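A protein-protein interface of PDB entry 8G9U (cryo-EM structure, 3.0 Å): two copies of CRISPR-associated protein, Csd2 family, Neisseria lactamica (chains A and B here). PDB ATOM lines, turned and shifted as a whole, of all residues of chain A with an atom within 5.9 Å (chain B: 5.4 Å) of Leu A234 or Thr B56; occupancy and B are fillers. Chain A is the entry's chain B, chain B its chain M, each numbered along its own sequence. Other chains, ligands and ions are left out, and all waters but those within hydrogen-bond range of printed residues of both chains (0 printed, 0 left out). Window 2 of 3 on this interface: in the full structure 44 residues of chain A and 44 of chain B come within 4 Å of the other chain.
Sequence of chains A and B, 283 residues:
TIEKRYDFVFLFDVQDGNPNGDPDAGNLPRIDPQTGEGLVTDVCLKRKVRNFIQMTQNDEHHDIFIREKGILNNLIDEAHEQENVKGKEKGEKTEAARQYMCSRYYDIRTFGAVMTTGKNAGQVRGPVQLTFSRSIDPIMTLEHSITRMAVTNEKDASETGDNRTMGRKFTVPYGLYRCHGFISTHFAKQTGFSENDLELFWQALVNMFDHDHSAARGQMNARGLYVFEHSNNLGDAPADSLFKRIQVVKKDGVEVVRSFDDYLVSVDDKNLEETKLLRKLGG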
ATOM      1  N   ARG A   5      -0.880  -4.666   6.268  1.00  0.00           N
ATOM      2  CA  ARG A   5      -0.243  -4.091   5.090  1.00  0.00           C
ATOM      3  C   ARG A   5      -1.230  -4.154   3.944  1.00  0.00           C
ATOM      4  O   ARG A   5      -1.768  -5.221   3.646  1.00  0.00           O
ATOM      5  CB  ARG A   5       1.038  -4.820   4.712  1.00  0.00           C
ATOM      6  CG  ARG A   5       1.763  -4.129   3.583  1.00  0.00           C
ATOM      7  CD  ARG A   5       3.078  -4.788   3.266  1.00  0.00           C
ATOM      8  NE  ARG A   5       2.926  -5.823   2.253  1.00  0.00           N
ATOM      9  CZ  ARG A   5       2.719  -5.578   0.967  1.00  0.00           C
ATOM     10  NH1 ARG A   5       2.600  -6.582   0.111  1.00  0.00           N
ATOM     11  NH2 ARG A   5       2.639  -4.329   0.532  1.00  0.00           N
ATOM     12  N   THR A 185       2.978  -1.202   6.385  1.00  0.00           N
ATOM     13  CA  THR A 185       2.920  -1.031   7.825  1.00  0.00           C
ATOM     14  C   THR A 185       4.207  -0.446   8.365  1.00  0.00           C
ATOM     15  O   THR A 185       4.178   0.345   9.311  1.00  0.00           O
ATOM     16  CB  THR A 185       2.636  -2.362   8.497  1.00  0.00           C
ATOM     17  OG1 THR A 185       1.349  -2.822   8.088  1.00  0.00           O
ATOM     18  CG2 THR A 185       2.648  -2.210  10.000  1.00  0.00           C
ATOM     19  N   HIS A 186       5.342  -0.807   7.776  1.00  0.00           N
ATOM     20  CA  HIS A 186       6.612  -0.413   8.365  1.00  0.00           C
ATOM     21  C   HIS A 186       6.769   1.094   8.391  1.00  0.00           C
ATOM     22  O   HIS A 186       7.273   1.655   9.367  1.00  0.00           O
ATOM     23  CB  HIS A 186       7.772  -1.035   7.610  1.00  0.00           C
ATOM     24  CG  HIS A 186       9.098  -0.632   8.156  1.00  0.00           C
ATOM     25  ND1 HIS A 186       9.641  -1.210   9.280  1.00  0.00           N
ATOM     26  CD2 HIS A 186       9.974   0.318   7.759  1.00  0.00           C
ATOM     27  CE1 HIS A 186      10.807  -0.648   9.541  1.00  0.00           C
ATOM     28  NE2 HIS A 186      11.031   0.281   8.631  1.00  0.00           N
ATOM     29  N   HIS A 230      -3.424  -7.505   4.208  1.00  0.00           N
ATOM     30  CA  HIS A 230      -2.718  -8.730   4.545  1.00  0.00           C
ATOM     31  C   HIS A 230      -2.706  -8.919   6.050  1.00  0.00           C
ATOM     32  O   HIS A 230      -2.640  -7.950   6.809  1.00  0.00           O
ATOM     33  CB  HIS A 230      -1.283  -8.702   4.027  1.00  0.00           C
ATOM     34  CG  HIS A 230      -1.151  -8.227   2.618  1.00  0.00           C
ATOM     35  ND1 HIS A 230       0.056  -7.851   2.076  1.00  0.00           N
ATOM     36  CD2 HIS A 230      -2.076  -8.017   1.656  1.00  0.00           C
ATOM     37  CE1 HIS A 230      -0.125  -7.469   0.826  1.00  0.00           C
ATOM     38  NE2 HIS A 230      -1.410  -7.559   0.547  1.00  0.00           N
ATOM     39  N   SER A 231      -2.752 -10.176   6.482  1.00  0.00           N
ATOM     40  CA  SER A 231      -2.842 -10.443   7.909  1.00  0.00           C
ATOM     41  C   SER A 231      -1.604  -9.959   8.640  1.00  0.00           C
ATOM     42  O   SER A 231      -1.679  -9.555   9.804  1.00  0.00           O
ATOM     43  CB  SER A 231      -3.044 -11.930   8.151  1.00  0.00           C
ATOM     44  OG  SER A 231      -2.149 -12.687   7.364  1.00  0.00           O
ATOM     45  N   ASN A 232      -0.456 -10.002   7.988  1.00  0.00           N
ATOM     46  CA  ASN A 232       0.765  -9.601   8.658  1.00  0.00           C
ATOM     47  C   ASN A 232       1.195  -8.214   8.201  1.00  0.00           C
ATOM     48  O   ASN A 232       0.811  -7.736   7.135  1.00  0.00           O
ATOM     49  CB  ASN A 232       1.880 -10.615   8.402  1.00  0.00           C
ATOM     50  CG  ASN A 232       2.013 -10.980   6.940  1.00  0.00           C
ATOM     51  OD1 ASN A 232       1.432 -10.340   6.069  1.00  0.00           O
ATOM     52  ND2 ASN A 232       2.781 -12.024   6.663  1.00  0.00           N
ATOM     53  N   ASN A 233       1.992  -7.561   9.042  1.00  0.00           N
ATOM     54  CA  ASN A 233       2.678  -6.358   8.601  1.00  0.00           C
ATOM     55  C   ASN A 233       3.687  -6.659   7.503  1.00  0.00           C
ATOM     56  O   ASN A 233       4.145  -5.739   6.819  1.00  0.00           O
ATOM     57  CB  ASN A 233       3.319  -5.670   9.807  1.00  0.00           C
ATOM     58  CG  ASN A 233       4.383  -6.511  10.473  1.00  0.00           C
ATOM     59  OD1 ASN A 233       4.754  -7.574   9.985  1.00  0.00           O
ATOM     60  ND2 ASN A 233       4.869  -6.042  11.613  1.00  0.00           N
ATOM     61  N   LEU A 234       4.030  -7.929   7.317  1.00  0.00           N
ATOM     62  CA  LEU A 234       4.704  -8.400   6.117  1.00  0.00           C
ATOM     63  C   LEU A 234       3.661  -8.525   5.013  1.00  0.00           C
ATOM     64  O   LEU A 234       2.544  -8.017   5.121  1.00  0.00           O
ATOM     65  CB  LEU A 234       5.401  -9.733   6.371  1.00  0.00           C
ATOM     66  CG  LEU A 234       6.800  -9.809   6.982  1.00  0.00           C
ATOM     67  CD1 LEU A 234       7.828  -9.183   6.064  1.00  0.00           C
ATOM     68  CD2 LEU A 234       6.846  -9.173   8.355  1.00  0.00           C
ATOM     69  N   GLY A 235       4.014  -9.196   3.927  1.00  0.00           N
ATOM     70  CA  GLY A 235       3.037  -9.455   2.894  1.00  0.00           C
ATOM     71  C   GLY A 235       2.566 -10.891   2.895  1.00  0.00           C
ATOM     72  O   GLY A 235       3.382 -11.811   2.819  1.00  0.00           O
ATOM     73  N   ASP A 236       1.252 -11.102   2.988  1.00  0.00           N
ATOM     74  CA  ASP A 236       0.722 -12.457   2.885  1.00  0.00           C
ATOM     75  C   ASP A 236       1.043 -13.065   1.530  1.00  0.00           C
ATOM     76  O   ASP A 236       1.360 -14.254   1.432  1.00  0.00           O
ATOM     77  CB  ASP A 236      -0.785 -12.460   3.122  1.00  0.00           C
ATOM     78  CG  ASP A 236      -1.143 -12.332   4.583  1.00  0.00           C
ATOM     79  OD1 ASP A 236      -0.327 -12.749   5.430  1.00  0.00           O
ATOM     80  OD2 ASP A 236      -2.244 -11.829   4.889  1.00  0.00           O
ATOM     81  N   ASN B  51      17.176  -3.160   3.469  1.00  0.00           N
ATOM     82  CA  ASN B  51      15.970  -2.561   4.012  1.00  0.00           C
ATOM     83  C   ASN B  51      15.008  -3.621   4.500  1.00  0.00           C
ATOM     84  O   ASN B  51      14.486  -3.522   5.610  1.00  0.00           O
ATOM     85  CB  ASN B  51      15.308  -1.687   2.967  1.00  0.00           C
ATOM     86  CG  ASN B  51      16.092  -0.468   2.698  1.00  0.00           C
ATOM     87  OD1 ASN B  51      16.922  -0.083   3.509  1.00  0.00           O
ATOM     88  ND2 ASN B  51      15.839   0.172   1.567  1.00  0.00           N
ATOM     89  N   PHE B  52      14.774  -4.656   3.698  1.00  0.00           N
ATOM     90  CA  PHE B  52      13.846  -5.690   4.129  1.00  0.00           C
ATOM     91  C   PHE B  52      14.305  -6.322   5.428  1.00  0.00           C
ATOM     92  O   PHE B  52      13.531  -6.446   6.380  1.00  0.00           O
ATOM     93  CB  PHE B  52      13.693  -6.762   3.065  1.00  0.00           C
ATOM     94  CG  PHE B  52      12.945  -7.951   3.550  1.00  0.00           C
ATOM     95  CD1 PHE B  52      11.580  -7.919   3.652  1.00  0.00           C
ATOM     96  CD2 PHE B  52      13.609  -9.076   3.971  1.00  0.00           C
ATOM     97  CE1 PHE B  52      10.888  -9.006   4.102  1.00  0.00           C
ATOM     98  CE2 PHE B  52      12.923 -10.163   4.436  1.00  0.00           C
ATOM     99  CZ  PHE B  52      11.560 -10.128   4.504  1.00  0.00           C
ATOM    100  N   ILE B  53      15.571  -6.724   5.491  1.00  0.00           N
ATOM    101  CA  ILE B  53      16.060  -7.346   6.704  1.00  0.00           C
ATOM    102  C   ILE B  53      16.001  -6.382   7.866  1.00  0.00           C
ATOM    103  O   ILE B  53      15.909  -6.805   9.022  1.00  0.00           O
ATOM    104  CB  ILE B  53      17.479  -7.874   6.492  1.00  0.00           C
ATOM    105  CG1 ILE B  53      17.493  -8.843   5.318  1.00  0.00           C
ATOM    106  CG2 ILE B  53      17.955  -8.565   7.727  1.00  0.00           C
ATOM    107  CD1 ILE B  53      16.665 -10.072   5.539  1.00  0.00           C
ATOM    108  N   GLN B  54      16.031  -5.087   7.598  1.00  0.00           N
ATOM    109  CA  GLN B  54      15.861  -4.138   8.684  1.00  0.00           C
ATOM    110  C   GLN B  54      14.410  -4.003   9.117  1.00  0.00           C
ATOM    111  O   GLN B  54      14.141  -3.802  10.305  1.00  0.00           O
ATOM    112  CB  GLN B  54      16.415  -2.782   8.274  1.00  0.00           C
ATOM    113  CG  GLN B  54      16.549  -1.842   9.414  1.00  0.00           C
ATOM    114  CD  GLN B  54      17.354  -0.647   9.041  1.00  0.00           C
ATOM    115  OE1 GLN B  54      17.941  -0.600   7.964  1.00  0.00           O
ATOM    116  NE2 GLN B  54      17.385   0.341   9.919  1.00  0.00           N
ATOM    117  N   MET B  55      13.472  -4.115   8.181  1.00  0.00           N
ATOM    118  CA  MET B  55      12.058  -4.027   8.522  1.00  0.00           C
ATOM    119  C   MET B  55      11.609  -5.240   9.312  1.00  0.00           C
ATOM    120  O   MET B  55      10.952  -5.115  10.350  1.00  0.00           O
ATOM    121  CB  MET B  55      11.228  -3.928   7.251  1.00  0.00           C
ATOM    122  CG  MET B  55      11.690  -2.862   6.322  1.00  0.00           C
ATOM    123  SD  MET B  55      10.535  -2.517   5.008  1.00  0.00           S
ATOM    124  CE  MET B  55      11.209  -0.961   4.502  1.00  0.00           C
ATOM    125  N   THR B  56      11.964  -6.425   8.834  1.00  0.00           N
ATOM    126  CA  THR B  56      11.380  -7.673   9.292  1.00  0.00           C
ATOM    127  C   THR B  56      11.997  -8.178  10.587  1.00  0.00           C
ATOM    128  O   THR B  56      11.281  -8.612  11.491  1.00  0.00           O
ATOM    129  CB  THR B  56      11.531  -8.721   8.197  1.00  0.00           C
ATOM    130  OG1 THR B  56      10.900  -8.238   7.011  1.00  0.00           O
ATOM    131  CG2 THR B  56      10.878 -10.013   8.614  1.00  0.00           C
ATOM    132  N   GLN B  57      13.319  -8.127  10.694  1.00  0.00           N
ATOM    133  CA  GLN B  57      13.988  -8.822  11.785  1.00  0.00           C
ATOM    134  C   GLN B  57      13.825  -8.089  13.111  1.00  0.00           C
ATOM    135  O   GLN B  57      13.303  -8.655  14.080  1.00  0.00           O
ATOM    136  CB  GLN B  57      15.451  -9.010  11.431  1.00  0.00           C
ATOM    137  CG  GLN B  57      15.617  -9.763  10.141  1.00  0.00           C
ATOM    138  CD  GLN B  57      14.738 -10.984  10.086  1.00  0.00           C
ATOM    139  OE1 GLN B  57      13.843 -11.077   9.251  1.00  0.00           O
ATOM    140  NE2 GLN B  57      14.982 -11.930  10.981  1.00  0.00           N
ATOM    141  N   ASN B  58      14.278  -6.839  13.179  1.00  0.00           N
ATOM    142  CA  ASN B  58      14.107  -6.004  14.369  1.00  0.00           C
ATOM    143  C   ASN B  58      14.678  -6.673  15.615  1.00  0.00           C
ATOM    144  O   ASN B  58      14.078  -6.639  16.690  1.00  0.00           O
ATOM    145  CB  ASN B  58      12.632  -5.652  14.587  1.00  0.00           C
ATOM    146  CG  ASN B  58      12.115  -4.650  13.580  1.00  0.00           C
ATOM    147  OD1 ASN B  58      12.804  -3.697  13.227  1.00  0.00           O
ATOM    148  ND2 ASN B  58      10.890  -4.858  13.114  1.00  0.00           N
ATOM    149  N   HIS B 211       7.873  -4.355   0.138  1.00  0.00           N
ATOM    150  CA  HIS B 211       8.059  -3.532   1.318  1.00  0.00           C
ATOM    151  C   HIS B 211       8.816  -2.251   1.043  1.00  0.00           C
ATOM    152  O   HIS B 211       8.612  -1.266   1.756  1.00  0.00           O
ATOM    153  CB  HIS B 211       8.796  -4.332   2.393  1.00  0.00           C
ATOM    154  CG  HIS B 211       8.048  -5.543   2.834  1.00  0.00           C
ATOM    155  ND1 HIS B 211       7.855  -6.631   2.015  1.00  0.00           N
ATOM    156  CD2 HIS B 211       7.444  -5.841   4.005  1.00  0.00           C
ATOM    157  CE1 HIS B 211       7.158  -7.547   2.660  1.00  0.00           C
ATOM    158  NE2 HIS B 211       6.897  -7.093   3.871  1.00  0.00           N
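His A186 touches Met B55. CD1 of Leu A234 touches CE1 of Phe B52, at 3.6 Å. OG1 of Thr B56 touches CD1 of Leu A234, 3.4 Å away. NE2 of His B211 touches CD1 of Leu A234, at 3.2 Å. His B211 touches Gly A235 (NE2 to N, 3.6 Å).
Of the 10 printed residues of chain A, 3 touch a printed residue of chain B. Printed residues of chain A that touch a printed residue of chain B: His A186, Leu A234 and Gly A235. Hydrophobic or aromatic side chains of chain A within 4 Å of the printed part of chain B: His A186 and Leu A234. Printed residues of chain B that touch a printed residue of chain A: Phe B52, Met B55, Thr B56 and His B211. Hydrophobic or aromatic side chains of chain B that line the printed part of chain A: Phe B52, Met B55 and His B211. Among the printed residues, no Asp or Glu carboxylate lies within 4 Å of a Lys or Arg side-chain nitrogen of the other chain.
No position is printed for both chains. Of the 5 pairs that touch across the chains among the printed residues, none has its exchanged pair printed and touching as well.
The side-chain amide oxygen of Asn A232 lies close to the backbone carbonyl oxygen of Leu A234 (2.7 Å). The backbone carbonyl oxygen (O) of Phe B52 lies close to the side-chain hydroxyl (OG1) of Thr B56. ND2 of Asn B58 is in hydrogen-bond range of O of Met B55 (2.8 Å).
Leu A234 touches just these residues of chain B: Phe B52 (3.6 Å), Thr B56 (3.4 Å) and His B211 (3.2 Å). Thr B56 touches just one residue of chain A: Leu A234 (3.4 Å). Of the printed residues of chain A, Phe B52 touches Leu A234 (3.6 Å). Printed residues of chain A within 4 Å of Met B55: His A186. Ile B53 touches none of the printed residues of chain A. Ser A231 touches none of the printed residues of chain B. The nearest printed residue of chain A that does not touch His B211 is Asn A233 (4.3 Å).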
